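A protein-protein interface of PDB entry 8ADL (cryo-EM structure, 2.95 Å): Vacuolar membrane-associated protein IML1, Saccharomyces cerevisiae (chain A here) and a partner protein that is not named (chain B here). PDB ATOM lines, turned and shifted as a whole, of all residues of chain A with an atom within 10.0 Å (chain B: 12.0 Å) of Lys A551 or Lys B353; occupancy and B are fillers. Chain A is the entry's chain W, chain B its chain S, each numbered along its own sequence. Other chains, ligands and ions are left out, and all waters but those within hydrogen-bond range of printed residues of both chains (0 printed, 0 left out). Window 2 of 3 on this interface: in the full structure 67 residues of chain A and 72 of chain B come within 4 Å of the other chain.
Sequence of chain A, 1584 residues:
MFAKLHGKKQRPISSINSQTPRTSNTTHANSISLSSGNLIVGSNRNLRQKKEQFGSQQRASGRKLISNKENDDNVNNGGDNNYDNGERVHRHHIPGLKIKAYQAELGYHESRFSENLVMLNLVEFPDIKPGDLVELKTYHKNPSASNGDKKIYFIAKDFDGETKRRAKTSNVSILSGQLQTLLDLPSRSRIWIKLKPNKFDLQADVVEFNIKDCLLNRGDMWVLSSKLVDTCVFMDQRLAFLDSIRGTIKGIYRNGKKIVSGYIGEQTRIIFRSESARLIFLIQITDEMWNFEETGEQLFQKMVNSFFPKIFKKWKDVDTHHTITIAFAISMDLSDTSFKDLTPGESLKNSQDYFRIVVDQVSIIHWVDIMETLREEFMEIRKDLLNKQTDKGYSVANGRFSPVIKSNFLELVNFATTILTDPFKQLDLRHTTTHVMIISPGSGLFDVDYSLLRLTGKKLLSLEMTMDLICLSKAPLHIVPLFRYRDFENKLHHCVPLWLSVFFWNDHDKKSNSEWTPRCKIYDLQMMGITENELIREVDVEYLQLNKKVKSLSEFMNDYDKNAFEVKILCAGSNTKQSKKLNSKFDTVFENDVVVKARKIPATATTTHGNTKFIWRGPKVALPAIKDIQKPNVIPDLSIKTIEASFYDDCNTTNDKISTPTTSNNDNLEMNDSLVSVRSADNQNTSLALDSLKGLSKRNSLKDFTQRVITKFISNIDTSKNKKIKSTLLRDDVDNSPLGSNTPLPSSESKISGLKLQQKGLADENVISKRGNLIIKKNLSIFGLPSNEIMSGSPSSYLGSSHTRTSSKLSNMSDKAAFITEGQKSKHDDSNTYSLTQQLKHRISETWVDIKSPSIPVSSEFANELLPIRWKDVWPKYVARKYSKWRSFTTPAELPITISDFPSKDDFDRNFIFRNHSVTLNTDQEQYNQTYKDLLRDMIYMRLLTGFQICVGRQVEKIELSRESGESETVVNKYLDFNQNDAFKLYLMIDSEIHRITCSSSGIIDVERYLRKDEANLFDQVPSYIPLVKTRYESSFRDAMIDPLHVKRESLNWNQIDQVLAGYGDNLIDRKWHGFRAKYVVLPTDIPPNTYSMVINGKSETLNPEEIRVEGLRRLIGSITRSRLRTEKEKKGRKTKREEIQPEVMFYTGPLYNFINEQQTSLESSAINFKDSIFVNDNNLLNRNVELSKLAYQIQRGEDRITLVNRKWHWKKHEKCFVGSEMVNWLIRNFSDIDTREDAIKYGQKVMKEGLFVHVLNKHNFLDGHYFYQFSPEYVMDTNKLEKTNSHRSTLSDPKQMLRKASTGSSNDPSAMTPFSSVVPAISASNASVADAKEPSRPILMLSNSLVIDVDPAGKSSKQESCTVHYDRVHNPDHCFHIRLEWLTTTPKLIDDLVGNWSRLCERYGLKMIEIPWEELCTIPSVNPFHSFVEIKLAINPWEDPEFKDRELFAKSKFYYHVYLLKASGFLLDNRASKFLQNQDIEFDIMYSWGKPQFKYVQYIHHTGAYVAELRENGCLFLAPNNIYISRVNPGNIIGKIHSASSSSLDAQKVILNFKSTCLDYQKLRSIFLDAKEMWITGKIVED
OD1 of Asn B352 is in hydrogen-bond range of OG of Ser A554 (3.3 Å). O of Leu B351 is in hydrogen-bond range of OG of Ser A552 (2.4 Å). The backbone NH (N) of Leu A553 is in hydrogen-bond range of the backbone carbonyl oxygen (O) of Pro B350 (2.6 Å). The side-chain hydroxyl (OG) of Ser A554 sits at hydrogen-bond distance from the backbone carbonyl oxygen (O) of Leu B351. The backbone NH (N) of Leu A553 sits at hydrogen-bond distance from the backbone carbonyl oxygen (O) of Leu B351 (3.5 Å).
N of Ile B346 lies close to OG of Ser B344. The side-chain hydroxyl of Ser A552 lies within hydrogen-bond range of the backbone NH of Ser A554 (3.1 Å).
Val A550 touches Leu B349. Lys A551 touches Pro B350. Ser A552 touches Leu B349 (O to CD2, 3.4 Å). Ser A552 touches Pro B350 (CA to O, 3.4 Å). CA of Asn B352 touches OG of Ser A552, 3.4 Å away. Lys B353 touches Ser A552 (N to CB, 3.8 Å). CD1 of Leu A553 touches CG2 of Ile B346, 3.9 Å away. CD2 of Leu A553 touches CB of Tyr B459 (3.9 Å). Met A557 touches Lys B452 (SD to CG, 3.8 Å). Met A557 touches Tyr B455.
Lys A549 touches none of the printed residues of chain B. Of chain B, only Leu B349 comes within 4 Å of Val A550. No residue of chain B comes within 4 Å of Glu A555. Printed residues of chain B within 4 Å of Phe A556: Ile B346 (3.9 Å). Ser B347 touches none of the printed residues of chain A. Of chain A, only Lys A551 (3.4 Å), Ser A552 (3.4 Å) and Leu A553 (2.6 Å) come within 4 Å of Pro B350. Of the printed residues of chain A, Leu B351 touches Ser A552 (2.4 Å), Leu A553 (3.5 Å) and Ser A554 (2.7 Å). Of chain A, only Lys A551 (3.8 Å) and Ser A552 (3.8 Å) come within 4 Å of Lys B353. The nearest residue of chain A that does not touch Lys B353 is Glu A555 (5.5 Å). The nearest printed residue of chain A that does not touch Lys B452 is Ser A554 (4.7 Å).
Of the 15 printed residues of chain B, 10 touch a printed residue of chain A. Hydrophobic or aromatic side chains of chain B within 4 Å of the printed part of chain A: Ile B346, Leu B349, Pro B350, Leu B351, Tyr B455 and Tyr B459. Among the printed residues, 20 pairs touch across the chains. Among the printed residues, no Asp or Glu carboxylate lies within 4 Å of a Lys or Arg side-chain nitrogen of the other chain.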
ATOM      1  N   LEU A 546     -35.274  27.482  15.199  1.00  0.00           N
ATOM      2  CA  LEU A 546     -33.881  27.152  15.452  1.00  0.00           C
ATOM      3  C   LEU A 546     -33.148  26.859  14.143  1.00  0.00           C
ATOM      4  O   LEU A 546     -33.652  27.104  13.045  1.00  0.00           O
ATOM      5  CB  LEU A 546     -33.789  25.973  16.419  1.00  0.00           C
ATOM      6  CG  LEU A 546     -33.585  26.317  17.895  1.00  0.00           C
ATOM      7  CD1 LEU A 546     -33.278  25.063  18.695  1.00  0.00           C
ATOM      8  CD2 LEU A 546     -32.474  27.337  18.056  1.00  0.00           C
ATOM      9  N   ASN A 547     -31.933  26.323  14.266  1.00  0.00           N
ATOM     10  CA  ASN A 547     -31.060  26.047  13.137  1.00  0.00           C
ATOM     11  C   ASN A 547     -30.736  24.566  12.980  1.00  0.00           C
ATOM     12  O   ASN A 547     -30.235  24.173  11.918  1.00  0.00           O
ATOM     13  CB  ASN A 547     -29.752  26.847  13.275  1.00  0.00           C
ATOM     14  CG  ASN A 547     -28.973  26.936  11.975  1.00  0.00           C
ATOM     15  OD1 ASN A 547     -29.554  27.012  10.893  1.00  0.00           O
ATOM     16  ND2 ASN A 547     -27.648  26.925  12.078  1.00  0.00           N
ATOM     17  N   LYS A 548     -31.011  23.745  14.004  1.00  0.00           N
ATOM     18  CA  LYS A 548     -30.594  22.337  14.098  1.00  0.00           C
ATOM     19  C   LYS A 548     -29.075  22.189  14.000  1.00  0.00           C
ATOM     20  O   LYS A 548     -28.561  21.186  13.498  1.00  0.00           O
ATOM     21  CB  LYS A 548     -31.302  21.453  13.061  1.00  0.00           C
ATOM     22  CG  LYS A 548     -31.619  20.048  13.556  1.00  0.00           C
ATOM     23  CD  LYS A 548     -32.202  19.183  12.450  1.00  0.00           C
ATOM     24  CE  LYS A 548     -32.466  17.769  12.942  1.00  0.00           C
ATOM     25  NZ  LYS A 548     -32.944  16.880  11.847  1.00  0.00           N
ATOM     26  N   LYS A 549     -28.353  23.203  14.482  1.00  0.00           N
ATOM     27  CA  LYS A 549     -26.902  23.147  14.607  1.00  0.00           C
ATOM     28  C   LYS A 549     -26.433  23.821  15.890  1.00  0.00           C
ATOM     29  O   LYS A 549     -25.222  23.990  16.078  1.00  0.00           O
ATOM     30  CB  LYS A 549     -26.221  23.800  13.399  1.00  0.00           C
ATOM     31  CG  LYS A 549     -25.662  22.815  12.386  1.00  0.00           C
ATOM     32  CD  LYS A 549     -25.314  23.511  11.081  1.00  0.00           C
ATOM     33  CE  LYS A 549     -24.784  22.528  10.051  1.00  0.00           C
ATOM     34  NZ  LYS A 549     -24.455  23.201   8.763  1.00  0.00           N
ATOM     35  N   VAL A 550     -27.353  24.208  16.771  1.00  0.00           N
ATOM     36  CA  VAL A 550     -27.068  25.059  17.919  1.00  0.00           C
ATOM     37  C   VAL A 550     -27.454  24.301  19.182  1.00  0.00           C
ATOM     38  O   VAL A 550     -28.594  23.840  19.308  1.00  0.00           O
ATOM     39  CB  VAL A 550     -27.829  26.394  17.821  1.00  0.00           C
ATOM     40  CG1 VAL A 550     -27.753  27.149  19.125  1.00  0.00           C
ATOM     41  CG2 VAL A 550     -27.283  27.236  16.677  1.00  0.00           C
ATOM     42  N   LYS A 551     -26.505  24.171  20.111  1.00  0.00           N
ATOM     43  CA  LYS A 551     -26.720  23.428  21.346  1.00  0.00           C
ATOM     44  C   LYS A 551     -26.709  24.301  22.595  1.00  0.00           C
ATOM     45  O   LYS A 551     -26.903  23.778  23.698  1.00  0.00           O
ATOM     46  CB  LYS A 551     -25.666  22.323  21.491  1.00  0.00           C
ATOM     47  CG  LYS A 551     -25.329  21.595  20.199  1.00  0.00           C
ATOM     48  CD  LYS A 551     -26.511  20.779  19.702  1.00  0.00           C
ATOM     49  CE  LYS A 551     -26.275  20.270  18.290  1.00  0.00           C
ATOM     50  NZ  LYS A 551     -27.452  19.525  17.766  1.00  0.00           N
ATOM     51  N   SER A 552     -26.490  25.608  22.462  1.00  0.00           N
ATOM     52  CA  SER A 552     -26.426  26.501  23.609  1.00  0.00           C
ATOM     53  C   SER A 552     -27.232  27.762  23.331  1.00  0.00           C
ATOM     54  O   SER A 552     -27.388  28.177  22.180  1.00  0.00           O
ATOM     55  CB  SER A 552     -24.980  26.880  23.953  1.00  0.00           C
ATOM     56  OG  SER A 552     -24.941  28.039  24.766  1.00  0.00           O
ATOM     57  N   LEU A 553     -27.738  28.371  24.404  1.00  0.00           N
ATOM     58  CA  LEU A 553     -28.506  29.603  24.259  1.00  0.00           C
ATOM     59  C   LEU A 553     -27.609  30.772  23.867  1.00  0.00           C
ATOM     60  O   LEU A 553     -28.009  31.632  23.070  1.00  0.00           O
ATOM     61  CB  LEU A 553     -29.244  29.896  25.565  1.00  0.00           C
ATOM     62  CG  LEU A 553     -30.503  30.760  25.528  1.00  0.00           C
ATOM     63  CD1 LEU A 553     -31.578  30.090  24.689  1.00  0.00           C
ATOM     64  CD2 LEU A 553     -30.995  30.990  26.947  1.00  0.00           C
ATOM     65  N   SER A 554     -26.385  30.807  24.403  1.00  0.00           N
ATOM     66  CA  SER A 554     -25.419  31.829  24.010  1.00  0.00           C
ATOM     67  C   SER A 554     -25.004  31.669  22.553  1.00  0.00           C
ATOM     68  O   SER A 554     -24.830  32.665  21.839  1.00  0.00           O
ATOM     69  CB  SER A 554     -24.196  31.772  24.925  1.00  0.00           C
ATOM     70  OG  SER A 554     -24.581  31.708  26.288  1.00  0.00           O
ATOM     71  N   GLU A 555     -24.846  30.423  22.095  1.00  0.00           N
ATOM     72  CA  GLU A 555     -24.557  30.175  20.686  1.00  0.00           C
ATOM     73  C   GLU A 555     -25.723  30.592  19.796  1.00  0.00           C
ATOM     74  O   GLU A 555     -25.511  31.092  18.686  1.00  0.00           O
ATOM     75  CB  GLU A 555     -24.218  28.700  20.473  1.00  0.00           C
ATOM     76  CG  GLU A 555     -22.891  28.276  21.080  1.00  0.00           C
ATOM     77  CD  GLU A 555     -21.702  28.899  20.375  1.00  0.00           C
ATOM     78  OE1 GLU A 555     -21.751  29.042  19.135  1.00  0.00           O
ATOM     79  OE2 GLU A 555     -20.717  29.246  21.062  1.00  0.00           O
ATOM     80  N   PHE A 556     -26.958  30.399  20.271  1.00  0.00           N
ATOM     81  CA  PHE A 556     -28.126  30.865  19.526  1.00  0.00           C
ATOM     82  C   PHE A 556     -28.145  32.385  19.418  1.00  0.00           C
ATOM     83  O   PHE A 556     -28.449  32.933  18.350  1.00  0.00           O
ATOM     84  CB  PHE A 556     -29.413  30.359  20.173  1.00  0.00           C
ATOM     85  CG  PHE A 556     -30.658  30.943  19.569  1.00  0.00           C
ATOM     86  CD1 PHE A 556     -31.032  30.613  18.277  1.00  0.00           C
ATOM     87  CD2 PHE A 556     -31.452  31.821  20.290  1.00  0.00           C
ATOM     88  CE1 PHE A 556     -32.175  31.146  17.713  1.00  0.00           C
ATOM     89  CE2 PHE A 556     -32.598  32.361  19.731  1.00  0.00           C
ATOM     90  CZ  PHE A 556     -32.960  32.022  18.441  1.00  0.00           C
ATOM     91  N   MET A 557     -27.826  33.081  20.516  1.00  0.00           N
ATOM     92  CA  MET A 557     -27.769  34.541  20.482  1.00  0.00           C
ATOM     93  C   MET A 557     -26.663  35.032  19.554  1.00  0.00           C
ATOM     94  O   MET A 557     -26.851  36.005  18.814  1.00  0.00           O
ATOM     95  CB  MET A 557     -27.565  35.100  21.890  1.00  0.00           C
ATOM     96  CG  MET A 557     -28.718  34.846  22.841  1.00  0.00           C
ATOM     97  SD  MET A 557     -28.498  35.709  24.407  1.00  0.00           S
ATOM     98  CE  MET A 557     -27.855  34.392  25.436  1.00  0.00           C
ATOM     99  N   ASP A 559     -25.410  33.388  16.926  1.00  0.00           N
ATOM    100  CA  ASP A 559     -25.786  33.110  15.544  1.00  0.00           C
ATOM    101  C   ASP A 559     -26.913  34.015  15.068  1.00  0.00           C
ATOM    102  O   ASP A 559     -27.010  34.300  13.868  1.00  0.00           O
ATOM    103  CB  ASP A 559     -26.187  31.642  15.396  1.00  0.00           C
ATOM    104  CG  ASP A 559     -24.991  30.728  15.208  1.00  0.00           C
ATOM    105  OD1 ASP A 559     -23.966  31.193  14.668  1.00  0.00           O
ATOM    106  OD2 ASP A 559     -25.077  29.546  15.600  1.00  0.00           O
ATOM    107  N   SER B 344     -41.174  24.545  23.087  1.00  0.00           N
ATOM    108  CA  SER B 344     -40.195  24.781  22.039  1.00  0.00           C
ATOM    109  C   SER B 344     -38.824  24.243  22.441  1.00  0.00           C
ATOM    110  O   SER B 344     -38.545  23.977  23.614  1.00  0.00           O
ATOM    111  CB  SER B 344     -40.100  26.274  21.722  1.00  0.00           C
ATOM    112  OG  SER B 344     -39.330  26.955  22.697  1.00  0.00           O
ATOM    113  N   LYS B 345     -37.961  24.087  21.436  1.00  0.00           N
ATOM    114  CA  LYS B 345     -36.618  23.573  21.672  1.00  0.00           C
ATOM    115  C   LYS B 345     -35.726  24.599  22.357  1.00  0.00           C
ATOM    116  O   LYS B 345     -34.753  24.212  23.012  1.00  0.00           O
ATOM    117  CB  LYS B 345     -35.983  23.124  20.355  1.00  0.00           C
ATOM    118  CG  LYS B 345     -36.666  21.927  19.714  1.00  0.00           C
ATOM    119  CD  LYS B 345     -37.391  22.321  18.438  1.00  0.00           C
ATOM    120  CE  LYS B 345     -38.049  21.116  17.785  1.00  0.00           C
ATOM    121  NZ  LYS B 345     -38.818  21.497  16.569  1.00  0.00           N
ATOM    122  N   ILE B 346     -36.037  25.893  22.212  1.00  0.00           N
ATOM    123  CA  ILE B 346     -35.305  26.941  22.918  1.00  0.00           C
ATOM    124  C   ILE B 346     -35.486  26.789  24.423  1.00  0.00           C
ATOM    125  O   ILE B 346     -34.554  27.031  25.202  1.00  0.00           O
ATOM    126  CB  ILE B 346     -35.764  28.327  22.412  1.00  0.00           C
ATOM    127  CG1 ILE B 346     -35.495  28.451  20.907  1.00  0.00           C
ATOM    128  CG2 ILE B 346     -35.072  29.456  23.176  1.00  0.00           C
ATOM    129  CD1 ILE B 346     -35.580  29.867  20.361  1.00  0.00           C
ATOM    130  N   SER B 347     -36.656  26.317  24.854  1.00  0.00           N
ATOM    131  CA  SER B 347     -36.905  25.988  26.253  1.00  0.00           C
ATOM    132  C   SER B 347     -36.273  24.661  26.681  1.00  0.00           C
ATOM    133  O   SER B 347     -36.650  24.124  27.728  1.00  0.00           O
ATOM    134  CB  SER B 347     -38.412  25.952  26.522  1.00  0.00           C
ATOM    135  OG  SER B 347     -38.701  25.264  27.727  1.00  0.00           O
ATOM    136  N   ASN B 348     -35.357  24.104  25.887  1.00  0.00           N
ATOM    137  CA  ASN B 348     -34.545  22.975  26.309  1.00  0.00           C
ATOM    138  C   ASN B 348     -33.050  23.236  26.205  1.00  0.00           C
ATOM    139  O   ASN B 348     -32.270  22.481  26.797  1.00  0.00           O
ATOM    140  CB  ASN B 348     -34.885  21.729  25.476  1.00  0.00           C
ATOM    141  CG  ASN B 348     -36.350  21.352  25.563  1.00  0.00           C
ATOM    142  OD1 ASN B 348     -36.975  21.478  26.615  1.00  0.00           O
ATOM    143  ND2 ASN B 348     -36.909  20.891  24.450  1.00  0.00           N
ATOM    144  N   LEU B 349     -32.633  24.272  25.481  1.00  0.00           N
ATOM    145  CA  LEU B 349     -31.216  24.583  25.353  1.00  0.00           C
ATOM    146  C   LEU B 349     -30.668  25.152  26.661  1.00  0.00           C
ATOM    147  O   LEU B 349     -31.311  25.998  27.289  1.00  0.00           O
ATOM    148  CB  LEU B 349     -30.977  25.577  24.217  1.00  0.00           C
ATOM    149  CG  LEU B 349     -30.512  25.010  22.873  1.00  0.00           C
ATOM    150  CD1 LEU B 349     -31.572  24.133  22.233  1.00  0.00           C
ATOM    151  CD2 LEU B 349     -30.112  26.139  21.935  1.00  0.00           C
ATOM    152  N   PRO B 350     -29.492  24.713  27.092  1.00  0.00           N
ATOM    153  CA  PRO B 350     -28.814  25.373  28.209  1.00  0.00           C
ATOM    154  C   PRO B 350     -28.162  26.672  27.752  1.00  0.00           C
ATOM    155  O   PRO B 350     -28.049  26.960  26.561  1.00  0.00           O
ATOM    156  CB  PRO B 350     -27.767  24.346  28.644  1.00  0.00           C
ATOM    157  CG  PRO B 350     -27.457  23.592  27.396  1.00  0.00           C
ATOM    158  CD  PRO B 350     -28.727  23.560  26.582  1.00  0.00           C
ATOM    159  N   LEU B 351     -27.743  27.468  28.738  1.00  0.00           N
ATOM    160  CA  LEU B 351     -27.102  28.745  28.438  1.00  0.00           C
ATOM    161  C   LEU B 351     -25.735  28.540  27.796  1.00  0.00           C
ATOM    162  O   LEU B 351     -25.385  29.231  26.833  1.00  0.00           O
ATOM    163  CB  LEU B 351     -26.979  29.584  29.709  1.00  0.00           C
ATOM    164  CG  LEU B 351     -26.485  31.019  29.520  1.00  0.00           C
ATOM    165  CD1 LEU B 351     -27.541  31.862  28.824  1.00  0.00           C
ATOM    166  CD2 LEU B 351     -26.097  31.633  30.856  1.00  0.00           C
ATOM    167  N   ASN B 352     -24.954  27.595  28.313  1.00  0.00           N
ATOM    168  CA  ASN B 352     -23.632  27.298  27.783  1.00  0.00           C
ATOM    169  C   ASN B 352     -23.447  25.792  27.716  1.00  0.00           C
ATOM    170  O   ASN B 352     -23.884  25.064  28.612  1.00  0.00           O
ATOM    171  CB  ASN B 352     -22.527  27.928  28.641  1.00  0.00           C
ATOM    172  CG  ASN B 352     -22.159  29.326  28.183  1.00  0.00           C
ATOM    173  OD1 ASN B 352     -22.141  29.615  26.986  1.00  0.00           O
ATOM    174  ND2 ASN B 352     -21.864  30.203  29.136  1.00  0.00           N
ATOM    175  N   LYS B 353     -22.798  25.331  26.652  1.00  0.00           N
ATOM    176  CA  LYS B 353     -22.534  23.909  26.468  1.00  0.00           C
ATOM    177  C   LYS B 353     -21.307  23.694  25.588  1.00  0.00           C
ATOM    178  O   LYS B 353     -21.211  24.249  24.494  1.00  0.00           O
ATOM    179  CB  LYS B 353     -23.749  23.210  25.856  1.00  0.00           C
ATOM    180  CG  LYS B 353     -23.592  21.704  25.720  1.00  0.00           C
ATOM    181  CD  LYS B 353     -24.901  21.045  25.316  1.00  0.00           C
ATOM    182  CE  LYS B 353     -24.770  19.531  25.288  1.00  0.00           C
ATOM    183  NZ  LYS B 353     -26.059  18.868  24.947  1.00  0.00           N
ATOM    184  N   LYS B 452     -28.298  40.576  25.738  1.00  0.00           N
ATOM    185  CA  LYS B 452     -27.573  39.336  25.997  1.00  0.00           C
ATOM    186  C   LYS B 452     -27.354  39.133  27.491  1.00  0.00           C
ATOM    187  O   LYS B 452     -27.595  38.041  28.019  1.00  0.00           O
ATOM    188  CB  LYS B 452     -26.238  39.346  25.252  1.00  0.00           C
ATOM    189  CG  LYS B 452     -25.564  37.986  25.166  1.00  0.00           C
ATOM    190  CD  LYS B 452     -24.465  37.980  24.115  1.00  0.00           C
ATOM    191  CE  LYS B 452     -23.772  36.629  24.051  1.00  0.00           C
ATOM    192  NZ  LYS B 452     -22.631  36.635  23.094  1.00  0.00           N
ATOM    193  N   TYR B 455     -30.748  38.530  29.189  1.00  0.00           N
ATOM    194  CA  TYR B 455     -31.283  37.208  28.896  1.00  0.00           C
ATOM    195  C   TYR B 455     -30.477  36.104  29.565  1.00  0.00           C
ATOM    196  O   TYR B 455     -31.050  35.088  29.964  1.00  0.00           O
ATOM    197  CB  TYR B 455     -31.335  36.995  27.382  1.00  0.00           C
ATOM    198  CG  TYR B 455     -32.093  35.760  26.947  1.00  0.00           C
ATOM    199  CD1 TYR B 455     -33.232  35.341  27.626  1.00  0.00           C
ATOM    200  CD2 TYR B 455     -31.691  35.035  25.832  1.00  0.00           C
ATOM    201  CE1 TYR B 455     -33.930  34.217  27.223  1.00  0.00           C
ATOM    202  CE2 TYR B 455     -32.387  33.916  25.418  1.00  0.00           C
ATOM    203  CZ  TYR B 455     -33.504  33.510  26.118  1.00  0.00           C
ATOM    204  OH  TYR B 455     -34.198  32.394  25.709  1.00  0.00           O
ATOM    205  N   GLU B 456     -29.162  36.284  29.713  1.00  0.00           N
ATOM    206  CA  GLU B 456     -28.345  35.304  30.416  1.00  0.00           C
ATOM    207  C   GLU B 456     -28.420  35.449  31.930  1.00  0.00           C
ATOM    208  O   GLU B 456     -28.003  34.529  32.643  1.00  0.00           O
ATOM    209  CB  GLU B 456     -26.885  35.403  29.962  1.00  0.00           C
ATOM    210  CG  GLU B 456     -26.104  36.546  30.587  1.00  0.00           C
ATOM    211  CD  GLU B 456     -24.838  36.876  29.820  1.00  0.00           C
ATOM    212  OE1 GLU B 456     -24.598  36.248  28.767  1.00  0.00           O
ATOM    213  OE2 GLU B 456     -24.082  37.763  30.270  1.00  0.00           O
ATOM    214  N   TYR B 459     -32.721  33.441  32.330  1.00  0.00           N
ATOM    215  CA  TYR B 459     -32.996  32.451  31.299  1.00  0.00           C
ATOM    216  C   TYR B 459     -33.744  31.231  31.806  1.00  0.00           C
ATOM    217  O   TYR B 459     -34.429  30.583  31.015  1.00  0.00           O
ATOM    218  CB  TYR B 459     -31.690  31.989  30.625  1.00  0.00           C
ATOM    219  CG  TYR B 459     -30.871  30.999  31.424  1.00  0.00           C
ATOM    220  CD1 TYR B 459     -30.186  31.393  32.568  1.00  0.00           C
ATOM    221  CD2 TYR B 459     -30.766  29.672  31.020  1.00  0.00           C
ATOM    222  CE1 TYR B 459     -29.432  30.490  33.296  1.00  0.00           C
ATOM    223  CE2 TYR B 459     -30.012  28.763  31.741  1.00  0.00           C
ATOM    224  CZ  TYR B 459     -29.348  29.178  32.877  1.00  0.00           C
ATOM    225  OH  TYR B 459     -28.598  28.277  33.597  1.00  0.00           O
ATOM    226  N   LYS B 463     -37.243  29.933  30.175  1.00  0.00           N
ATOM    227  CA  LYS B 463     -37.254  28.536  29.765  1.00  0.00           C
ATOM    228  C   LYS B 463     -38.404  27.795  30.433  1.00  0.00           C
ATOM    229  O   LYS B 463     -39.099  27.000  29.789  1.00  0.00           O
ATOM    230  CB  LYS B 463     -35.916  27.882  30.110  1.00  0.00           C
ATOM    231  CG  LYS B 463     -35.851  26.396  29.846  1.00  0.00           C
ATOM    232  CD  LYS B 463     -34.430  25.871  29.962  1.00  0.00           C
ATOM    233  CE  LYS B 463     -33.980  25.813  31.411  1.00  0.00           C
ATOM    234  NZ  LYS B 463     -32.637  25.186  31.551  1.00  0.00           N
